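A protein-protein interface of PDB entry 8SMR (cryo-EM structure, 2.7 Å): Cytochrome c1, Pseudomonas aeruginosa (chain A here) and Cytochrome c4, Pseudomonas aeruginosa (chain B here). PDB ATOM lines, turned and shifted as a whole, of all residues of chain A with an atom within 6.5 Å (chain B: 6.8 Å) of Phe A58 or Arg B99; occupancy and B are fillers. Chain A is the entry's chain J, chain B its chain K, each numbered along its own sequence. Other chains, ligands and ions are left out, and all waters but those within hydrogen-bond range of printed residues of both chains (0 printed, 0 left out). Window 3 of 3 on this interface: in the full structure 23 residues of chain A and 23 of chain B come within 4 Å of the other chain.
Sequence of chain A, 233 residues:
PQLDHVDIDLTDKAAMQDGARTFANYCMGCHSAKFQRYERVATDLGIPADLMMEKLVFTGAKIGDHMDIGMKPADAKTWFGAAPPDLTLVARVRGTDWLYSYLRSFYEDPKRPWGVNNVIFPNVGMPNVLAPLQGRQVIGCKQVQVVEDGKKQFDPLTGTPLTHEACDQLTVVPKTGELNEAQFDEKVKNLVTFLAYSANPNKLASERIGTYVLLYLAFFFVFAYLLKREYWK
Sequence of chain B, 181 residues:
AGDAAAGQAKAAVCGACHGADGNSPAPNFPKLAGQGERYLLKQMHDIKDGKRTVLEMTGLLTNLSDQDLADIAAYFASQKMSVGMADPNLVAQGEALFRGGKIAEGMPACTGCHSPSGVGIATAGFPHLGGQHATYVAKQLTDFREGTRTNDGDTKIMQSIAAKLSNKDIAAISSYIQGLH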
ATOM      1  N   ARG A  21      28.372   6.575  -7.804  1.00  0.00           N
ATOM      2  CA  ARG A  21      28.323   7.170  -9.136  1.00  0.00           C
ATOM      3  C   ARG A  21      28.004   6.115 -10.189  1.00  0.00           C
ATOM      4  O   ARG A  21      27.142   6.319 -11.058  1.00  0.00           O
ATOM      5  CB  ARG A  21      29.653   7.864  -9.431  1.00  0.00           C
ATOM      6  CG  ARG A  21      29.742   8.539 -10.788  1.00  0.00           C
ATOM      7  CD  ARG A  21      30.763   7.850 -11.677  1.00  0.00           C
ATOM      8  NE  ARG A  21      31.178   8.690 -12.794  1.00  0.00           N
ATOM      9  CZ  ARG A  21      31.873   8.258 -13.837  1.00  0.00           C
ATOM     10  NH1 ARG A  21      32.260   6.997 -13.936  1.00  0.00           N
ATOM     11  NH2 ARG A  21      32.193   9.114 -14.803  1.00  0.00           N
ATOM     12  N   ALA A  24      24.338   5.191  -9.852  1.00  0.00           N
ATOM     13  CA  ALA A  24      23.422   6.229 -10.307  1.00  0.00           C
ATOM     14  C   ALA A  24      23.409   6.325 -11.824  1.00  0.00           C
ATOM     15  O   ALA A  24      22.385   6.677 -12.421  1.00  0.00           O
ATOM     16  CB  ALA A  24      23.805   7.572  -9.690  1.00  0.00           C
ATOM     17  N   ASN A  25      24.537   6.020 -12.470  1.00  0.00           N
ATOM     18  CA  ASN A  25      24.617   6.198 -13.917  1.00  0.00           C
ATOM     19  C   ASN A  25      24.238   4.926 -14.672  1.00  0.00           C
ATOM     20  O   ASN A  25      23.335   4.939 -15.513  1.00  0.00           O
ATOM     21  CB  ASN A  25      26.023   6.656 -14.303  1.00  0.00           C
ATOM     22  CG  ASN A  25      26.271   8.107 -13.954  1.00  0.00           C
ATOM     23  OD1 ASN A  25      25.908   9.006 -14.708  1.00  0.00           O
ATOM     24  ND2 ASN A  25      26.883   8.342 -12.803  1.00  0.00           N
ATOM     25  N   MET A  28      20.719   2.724 -12.104  1.00  0.00           N
ATOM     26  CA  MET A  28      19.400   3.228 -11.757  1.00  0.00           C
ATOM     27  C   MET A  28      18.508   3.417 -12.974  1.00  0.00           C
ATOM     28  O   MET A  28      17.354   3.824 -12.816  1.00  0.00           O
ATOM     29  CB  MET A  28      19.533   4.536 -10.980  1.00  0.00           C
ATOM     30  CG  MET A  28      19.813   4.316  -9.501  1.00  0.00           C
ATOM     31  SD  MET A  28      19.626   5.788  -8.483  1.00  0.00           S
ATOM     32  CE  MET A  28      17.861   6.051  -8.595  1.00  0.00           C
ATOM     33  N   GLY A  29      19.010   3.137 -14.177  1.00  0.00           N
ATOM     34  CA  GLY A  29      18.134   3.105 -15.334  1.00  0.00           C
ATOM     35  C   GLY A  29      17.060   2.042 -15.212  1.00  0.00           C
ATOM     36  O   GLY A  29      15.907   2.266 -15.588  1.00  0.00           O
ATOM     37  N   TYR A  38      18.579   9.447  -0.729  1.00  0.00           N
ATOM     38  CA  TYR A  38      19.759  10.174  -1.188  1.00  0.00           C
ATOM     39  C   TYR A  38      20.426  10.909  -0.035  1.00  0.00           C
ATOM     40  O   TYR A  38      21.657  11.004   0.022  1.00  0.00           O
ATOM     41  CB  TYR A  38      19.380  11.169  -2.286  1.00  0.00           C
ATOM     42  CG  TYR A  38      18.871  10.558  -3.570  1.00  0.00           C
ATOM     43  CD1 TYR A  38      19.742   9.966  -4.474  1.00  0.00           C
ATOM     44  CD2 TYR A  38      17.523  10.598  -3.891  1.00  0.00           C
ATOM     45  CE1 TYR A  38      19.281   9.424  -5.657  1.00  0.00           C
ATOM     46  CE2 TYR A  38      17.052  10.054  -5.068  1.00  0.00           C
ATOM     47  CZ  TYR A  38      17.935   9.468  -5.947  1.00  0.00           C
ATOM     48  OH  TYR A  38      17.466   8.927  -7.119  1.00  0.00           O
ATOM     49  N   MET A  52      25.600  15.896  -3.898  1.00  0.00           N
ATOM     50  CA  MET A  52      24.739  14.742  -4.127  1.00  0.00           C
ATOM     51  C   MET A  52      23.589  15.102  -5.058  1.00  0.00           C
ATOM     52  O   MET A  52      23.259  14.344  -5.977  1.00  0.00           O
ATOM     53  CB  MET A  52      24.202  14.218  -2.795  1.00  0.00           C
ATOM     54  CG  MET A  52      23.379  12.943  -2.904  1.00  0.00           C
ATOM     55  SD  MET A  52      24.400  11.461  -2.914  1.00  0.00           S
ATOM     56  CE  MET A  52      23.178  10.207  -3.281  1.00  0.00           C
ATOM     57  N   MET A  53      22.972  16.263  -4.834  1.00  0.00           N
ATOM     58  CA  MET A  53      21.878  16.704  -5.691  1.00  0.00           C
ATOM     59  C   MET A  53      22.340  16.868  -7.130  1.00  0.00           C
ATOM     60  O   MET A  53      21.651  16.447  -8.066  1.00  0.00           O
ATOM     61  CB  MET A  53      21.318  18.028  -5.164  1.00  0.00           C
ATOM     62  CG  MET A  53      20.219  17.930  -4.108  1.00  0.00           C
ATOM     63  SD  MET A  53      19.118  16.516  -4.265  1.00  0.00           S
ATOM     64  CE  MET A  53      17.915  17.209  -5.387  1.00  0.00           C
ATOM     65  N   GLU A  54      23.510  17.475  -7.327  1.00  0.00           N
ATOM     66  CA  GLU A  54      23.960  17.802  -8.674  1.00  0.00           C
ATOM     67  C   GLU A  54      24.457  16.573  -9.426  1.00  0.00           C
ATOM     68  O   GLU A  54      24.289  16.485 -10.648  1.00  0.00           O
ATOM     69  CB  GLU A  54      25.057  18.868  -8.604  1.00  0.00           C
ATOM     70  CG  GLU A  54      25.943  18.952  -9.836  1.00  0.00           C
ATOM     71  CD  GLU A  54      26.951  20.080  -9.748  1.00  0.00           C
ATOM     72  OE1 GLU A  54      27.125  20.805 -10.749  1.00  0.00           O
ATOM     73  OE2 GLU A  54      27.571  20.241  -8.674  1.00  0.00           O
ATOM     74  N   LYS A  55      25.064  15.616  -8.725  1.00  0.00           N
ATOM     75  CA  LYS A  55      25.838  14.566  -9.373  1.00  0.00           C
ATOM     76  C   LYS A  55      25.173  13.199  -9.377  1.00  0.00           C
ATOM     77  O   LYS A  55      25.409  12.423 -10.305  1.00  0.00           O
ATOM     78  CB  LYS A  55      27.209  14.434  -8.701  1.00  0.00           C
ATOM     79  CG  LYS A  55      27.995  15.735  -8.616  1.00  0.00           C
ATOM     80  CD  LYS A  55      28.965  15.881  -9.776  1.00  0.00           C
ATOM     81  CE  LYS A  55      29.175  17.340 -10.141  1.00  0.00           C
ATOM     82  NZ  LYS A  55      30.456  17.562 -10.864  1.00  0.00           N
ATOM     83  N   LEU A  56      24.354  12.874  -8.374  1.00  0.00           N
ATOM     84  CA  LEU A  56      23.797  11.535  -8.250  1.00  0.00           C
ATOM     85  C   LEU A  56      22.281  11.471  -8.348  1.00  0.00           C
ATOM     86  O   LEU A  56      21.752  10.393  -8.637  1.00  0.00           O
ATOM     87  CB  LEU A  56      24.229  10.896  -6.919  1.00  0.00           C
ATOM     88  CG  LEU A  56      25.729  10.613  -6.792  1.00  0.00           C
ATOM     89  CD1 LEU A  56      26.082  10.146  -5.390  1.00  0.00           C
ATOM     90  CD2 LEU A  56      26.176   9.590  -7.816  1.00  0.00           C
ATOM     91  N   VAL A  57      21.570  12.575  -8.125  1.00  0.00           N
ATOM     92  CA  VAL A  57      20.113  12.592  -8.213  1.00  0.00           C
ATOM     93  C   VAL A  57      19.754  13.045  -9.625  1.00  0.00           C
ATOM     94  O   VAL A  57      19.833  14.230  -9.950  1.00  0.00           O
ATOM     95  CB  VAL A  57      19.492  13.499  -7.149  1.00  0.00           C
ATOM     96  CG1 VAL A  57      17.977  13.349  -7.143  1.00  0.00           C
ATOM     97  CG2 VAL A  57      20.071  13.185  -5.783  1.00  0.00           C
ATOM     98  N   PHE A  58      19.351  12.093 -10.467  1.00  0.00           N
ATOM     99  CA  PHE A  58      18.980  12.378 -11.846  1.00  0.00           C
ATOM    100  C   PHE A  58      17.474  12.416 -12.065  1.00  0.00           C
ATOM    101  O   PHE A  58      17.031  12.865 -13.127  1.00  0.00           O
ATOM    102  CB  PHE A  58      19.582  11.326 -12.786  1.00  0.00           C
ATOM    103  CG  PHE A  58      21.078  11.229 -12.720  1.00  0.00           C
ATOM    104  CD1 PHE A  58      21.858  12.362 -12.560  1.00  0.00           C
ATOM    105  CD2 PHE A  58      21.704  10.000 -12.821  1.00  0.00           C
ATOM    106  CE1 PHE A  58      23.232  12.266 -12.501  1.00  0.00           C
ATOM    107  CE2 PHE A  58      23.077   9.901 -12.761  1.00  0.00           C
ATOM    108  CZ  PHE A  58      23.842  11.034 -12.602  1.00  0.00           C
ATOM    109  N   THR A  59      16.682  11.965 -11.097  1.00  0.00           N
ATOM    110  CA  THR A  59      15.254  11.752 -11.283  1.00  0.00           C
ATOM    111  C   THR A  59      14.411  12.940 -10.838  1.00  0.00           C
ATOM    112  O   THR A  59      13.180  12.844 -10.836  1.00  0.00           O
ATOM    113  CB  THR A  59      14.812  10.498 -10.529  1.00  0.00           C
ATOM    114  OG1 THR A  59      14.885  10.733  -9.118  1.00  0.00           O
ATOM    115  CG2 THR A  59      15.700   9.317 -10.885  1.00  0.00           C
ATOM    116  N   GLY A  60      15.035  14.051 -10.463  1.00  0.00           N
ATOM    117  CA  GLY A  60      14.290  15.184  -9.961  1.00  0.00           C
ATOM    118  C   GLY A  60      13.778  15.016  -8.550  1.00  0.00           C
ATOM    119  O   GLY A  60      13.013  15.866  -8.080  1.00  0.00           O
ATOM    120  N   ALA A  61      14.173  13.948  -7.863  1.00  0.00           N
ATOM    121  CA  ALA A  61      13.755  13.724  -6.491  1.00  0.00           C
ATOM    122  C   ALA A  61      14.482  14.693  -5.564  1.00  0.00           C
ATOM    123  O   ALA A  61      15.488  15.306  -5.926  1.00  0.00           O
ATOM    124  CB  ALA A  61      14.028  12.278  -6.087  1.00  0.00           C
ATOM    125  N   GLY B  94      15.877  17.835 -21.505  1.00  0.00           N
ATOM    126  CA  GLY B  94      16.214  16.587 -22.165  1.00  0.00           C
ATOM    127  C   GLY B  94      17.126  15.717 -21.323  1.00  0.00           C
ATOM    128  O   GLY B  94      16.942  14.502 -21.247  1.00  0.00           O
ATOM    129  N   GLU B  95      18.120  16.331 -20.677  1.00  0.00           N
ATOM    130  CA  GLU B  95      19.015  15.582 -19.804  1.00  0.00           C
ATOM    131  C   GLU B  95      18.261  15.007 -18.615  1.00  0.00           C
ATOM    132  O   GLU B  95      18.483  13.853 -18.229  1.00  0.00           O
ATOM    133  CB  GLU B  95      20.150  16.485 -19.318  1.00  0.00           C
ATOM    134  CG  GLU B  95      21.127  15.791 -18.385  1.00  0.00           C
ATOM    135  CD  GLU B  95      22.380  16.604 -18.142  1.00  0.00           C
ATOM    136  OE1 GLU B  95      22.265  17.738 -17.632  1.00  0.00           O
ATOM    137  OE2 GLU B  95      23.482  16.109 -18.459  1.00  0.00           O
ATOM    138  N   ALA B  96      17.372  15.800 -18.013  1.00  0.00           N
ATOM    139  CA  ALA B  96      16.596  15.296 -16.888  1.00  0.00           C
ATOM    140  C   ALA B  96      15.757  14.097 -17.304  1.00  0.00           C
ATOM    141  O   ALA B  96      15.725  13.079 -16.604  1.00  0.00           O
ATOM    142  CB  ALA B  96      15.710  16.404 -16.321  1.00  0.00           C
ATOM    143  N   LEU B  97      15.088  14.190 -18.454  1.00  0.00           N
ATOM    144  CA  LEU B  97      14.270  13.073 -18.918  1.00  0.00           C
ATOM    145  C   LEU B  97      15.125  11.851 -19.230  1.00  0.00           C
ATOM    146  O   LEU B  97      14.761  10.724 -18.876  1.00  0.00           O
ATOM    147  CB  LEU B  97      13.463  13.491 -20.146  1.00  0.00           C
ATOM    148  CG  LEU B  97      12.289  14.428 -19.869  1.00  0.00           C
ATOM    149  CD1 LEU B  97      11.878  15.164 -21.132  1.00  0.00           C
ATOM    150  CD2 LEU B  97      11.116  13.654 -19.294  1.00  0.00           C
ATOM    151  N   PHE B  98      16.266  12.051 -19.892  1.00  0.00           N
ATOM    152  CA  PHE B  98      17.103  10.927 -20.296  1.00  0.00           C
ATOM    153  C   PHE B  98      17.682  10.206 -19.086  1.00  0.00           C
ATOM    154  O   PHE B  98      17.652   8.973 -19.013  1.00  0.00           O
ATOM    155  CB  PHE B  98      18.221  11.422 -21.216  1.00  0.00           C
ATOM    156  CG  PHE B  98      18.915  10.328 -21.977  1.00  0.00           C
ATOM    157  CD1 PHE B  98      19.979   9.641 -21.418  1.00  0.00           C
ATOM    158  CD2 PHE B  98      18.511   9.995 -23.259  1.00  0.00           C
ATOM    159  CE1 PHE B  98      20.619   8.637 -22.117  1.00  0.00           C
ATOM    160  CE2 PHE B  98      19.150   8.994 -23.963  1.00  0.00           C
ATOM    161  CZ  PHE B  98      20.203   8.314 -23.392  1.00  0.00           C
ATOM    162  N   ARG B  99      18.216  10.959 -18.123  1.00  0.00           N
ATOM    163  CA  ARG B  99      18.903  10.344 -16.994  1.00  0.00           C
ATOM    164  C   ARG B  99      17.945   9.865 -15.912  1.00  0.00           C
ATOM    165  O   ARG B  99      18.239   8.878 -15.231  1.00  0.00           O
ATOM    166  CB  ARG B  99      19.908  11.327 -16.396  1.00  0.00           C
ATOM    167  CG  ARG B  99      20.981  11.787 -17.366  1.00  0.00           C
ATOM    168  CD  ARG B  99      22.191  12.318 -16.622  1.00  0.00           C
ATOM    169  NE  ARG B  99      21.842  13.459 -15.786  1.00  0.00           N
ATOM    170  CZ  ARG B  99      22.707  14.358 -15.334  1.00  0.00           C
ATOM    171  NH1 ARG B  99      23.997  14.279 -15.615  1.00  0.00           N
ATOM    172  NH2 ARG B  99      22.266  15.358 -14.577  1.00  0.00           N
ATOM    173  N   GLY B 100      16.805  10.531 -15.740  1.00  0.00           N
ATOM    174  CA  GLY B 100      15.924  10.228 -14.631  1.00  0.00           C
ATOM    175  C   GLY B 100      14.591   9.633 -15.027  1.00  0.00           C
ATOM    176  O   GLY B 100      13.977   8.906 -14.242  1.00  0.00           O
ATOM    177  N   GLY B 101      14.129   9.930 -16.235  1.00  0.00           N
ATOM    178  CA  GLY B 101      12.811   9.475 -16.647  1.00  0.00           C
ATOM    179  C   GLY B 101      11.738  10.278 -15.949  1.00  0.00           C
ATOM    180  O   GLY B 101      11.885  11.485 -15.747  1.00  0.00           O
ATOM    181  N   PRO B 108      10.573   5.094 -17.733  1.00  0.00           N
ATOM    182  CA  PRO B 108      11.962   4.773 -17.398  1.00  0.00           C
ATOM    183  C   PRO B 108      12.923   5.832 -17.905  1.00  0.00           C
ATOM    184  O   PRO B 108      12.651   6.544 -18.875  1.00  0.00           O
ATOM    185  CB  PRO B 108      12.206   3.432 -18.102  1.00  0.00           C
ATOM    186  CG  PRO B 108      10.892   3.000 -18.650  1.00  0.00           C
ATOM    187  CD  PRO B 108      10.055   4.215 -18.792  1.00  0.00           C
ATOM    188  N   ALA B 109      14.057   5.937 -17.223  1.00  0.00           N
ATOM    189  CA  ALA B 109      15.175   6.684 -17.773  1.00  0.00           C
ATOM    190  C   ALA B 109      15.731   5.940 -18.978  1.00  0.00           C
ATOM    191  O   ALA B 109      15.668   4.710 -19.052  1.00  0.00           O
ATOM    192  CB  ALA B 109      16.264   6.874 -16.720  1.00  0.00           C
ATOM    193  N   CYS B 110      16.275   6.692 -19.930  1.00  0.00           N
ATOM    194  CA  CYS B 110      16.856   6.076 -21.113  1.00  0.00           C
ATOM    195  C   CYS B 110      18.241   5.509 -20.847  1.00  0.00           C
ATOM    196  O   CYS B 110      18.763   4.772 -21.689  1.00  0.00           O
ATOM    197  CB  CYS B 110      16.925   7.100 -22.243  1.00  0.00           C
ATOM    198  SG  CYS B 110      15.491   8.183 -22.311  1.00  0.00           S
ATOM    199  N   THR B 111      18.837   5.824 -19.695  1.00  0.00           N
ATOM    200  CA  THR B 111      20.206   5.418 -19.400  1.00  0.00           C
ATOM    201  C   THR B 111      20.335   3.933 -19.089  1.00  0.00           C
ATOM    202  O   THR B 111      21.456   3.417 -19.100  1.00  0.00           O
ATOM    203  CB  THR B 111      20.750   6.229 -18.228  1.00  0.00           C
ATOM    204  OG1 THR B 111      19.907   6.048 -17.083  1.00  0.00           O
ATOM    205  CG2 THR B 111      20.804   7.699 -18.590  1.00  0.00           C
ATOM    206  N   GLY B 112      19.235   3.240 -18.816  1.00  0.00           N
ATOM    207  CA  GLY B 112      19.307   1.820 -18.538  1.00  0.00           C
ATOM    208  C   GLY B 112      19.546   0.994 -19.783  1.00  0.00           C
ATOM    209  O   GLY B 112      20.596   0.365 -19.931  1.00  0.00           O
ATOM    210  N   PRO B 116      24.266   5.337 -20.206  1.00  0.00           N
ATOM    211  CA  PRO B 116      24.279   6.742 -19.771  1.00  0.00           C
ATOM    212  C   PRO B 116      24.923   7.658 -20.793  1.00  0.00           C
ATOM    213  O   PRO B 116      24.541   8.830 -20.901  1.00  0.00           O
ATOM    214  CB  PRO B 116      25.074   6.705 -18.456  1.00  0.00           C
ATOM    215  CG  PRO B 116      25.631   5.316 -18.336  1.00  0.00           C
ATOM    216  CD  PRO B 116      24.784   4.429 -19.172  1.00  0.00           C
ATOM    217  N   ILE B 173      14.423  15.828 -25.341  1.00  0.00           N
ATOM    218  CA  ILE B 173      15.251  14.638 -25.207  1.00  0.00           C
ATOM    219  C   ILE B 173      16.002  14.359 -26.502  1.00  0.00           C
ATOM    220  O   ILE B 173      17.151  13.910 -26.478  1.00  0.00           O
ATOM    221  CB  ILE B 173      14.397  13.437 -24.761  1.00  0.00           C
ATOM    222  CG1 ILE B 173      15.250  12.462 -23.949  1.00  0.00           C
ATOM    223  CG2 ILE B 173      13.776  12.726 -25.952  1.00  0.00           C
ATOM    224  CD1 ILE B 173      14.443  11.475 -23.151  1.00  0.00           C
ATOM    225  N   TYR B 176      18.914  16.733 -26.494  1.00  0.00           N
ATOM    226  CA  TYR B 176      19.943  16.251 -25.578  1.00  0.00           C
ATOM    227  C   TYR B 176      20.702  15.069 -26.170  1.00  0.00           C
ATOM    228  O   TYR B 176      21.930  14.990 -26.056  1.00  0.00           O
ATOM    229  CB  TYR B 176      19.314  15.861 -24.240  1.00  0.00           C
ATOM    230  CG  TYR B 176      20.270  15.144 -23.316  1.00  0.00           C
ATOM    231  CD1 TYR B 176      21.194  15.848 -22.561  1.00  0.00           C
ATOM    232  CD2 TYR B 176      20.252  13.761 -23.205  1.00  0.00           C
ATOM    233  CE1 TYR B 176      22.072  15.197 -21.717  1.00  0.00           C
ATOM    234  CE2 TYR B 176      21.125  13.102 -22.364  1.00  0.00           C
ATOM    235  CZ  TYR B 176      22.033  13.825 -21.621  1.00  0.00           C
ATOM    236  OH  TYR B 176      22.904  13.173 -20.782  1.00  0.00           O
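Phe A58 touches just these residues of chain B: Ala B96 (3.7 Å), Arg B99 (3.4 Å) and Gly B100 (3.2 Å). Arg B99 touches just one residue of chain A: Phe A58 (3.4 Å). Of the printed residues of chain A, Gly B100 touches Phe A58 and Thr A59. Of the printed residues of chain B, Gly A29 touches Thr B111 (3.9 Å) and Gly B112 (3.6 Å). Ala A61 touches none of the printed residues of chain B. The nearest residue of chain B that does not touch Phe A58 is Gly B101 (5.2 Å). The nearest residue of chain A that does not touch Arg B99 is Glu A54 (4.6 Å). The nearest printed residue of chain A that does not touch Thr B111 is Met A28 (5.1 Å).
Among the printed residues, pairs that only touch across the chains: Phe A58 with Gly B100 (3.2 Å), Phe A58 with Arg B99 (3.4 Å), Gly A29 with Gly B112 (3.6 Å), Asn A25 with Pro B116 (3.7 Å), Phe A58 with Ala B96 (3.7 Å), Thr A59 with Gly B100 (3.7 Å), Gly A29 with Thr B111 (3.9 Å) and Asn A25 with Thr B111 (3.9 Å).
The backbone carbonyl oxygen of Arg A21 lies within hydrogen-bond range of the side-chain amide nitrogen of Asn A25 (2.7 Å). The side-chain carboxylate of Glu B95 is in salt-bridge range of the guanidinium group of Arg B99. N of Thr B111 sits close to O of Phe B98 (3.4 Å).
Of the 16 printed residues of chain B, 6 touch a printed residue of chain A. Hydrophobic or aromatic side chains of chain B that line the printed part of chain A: Pro B116.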
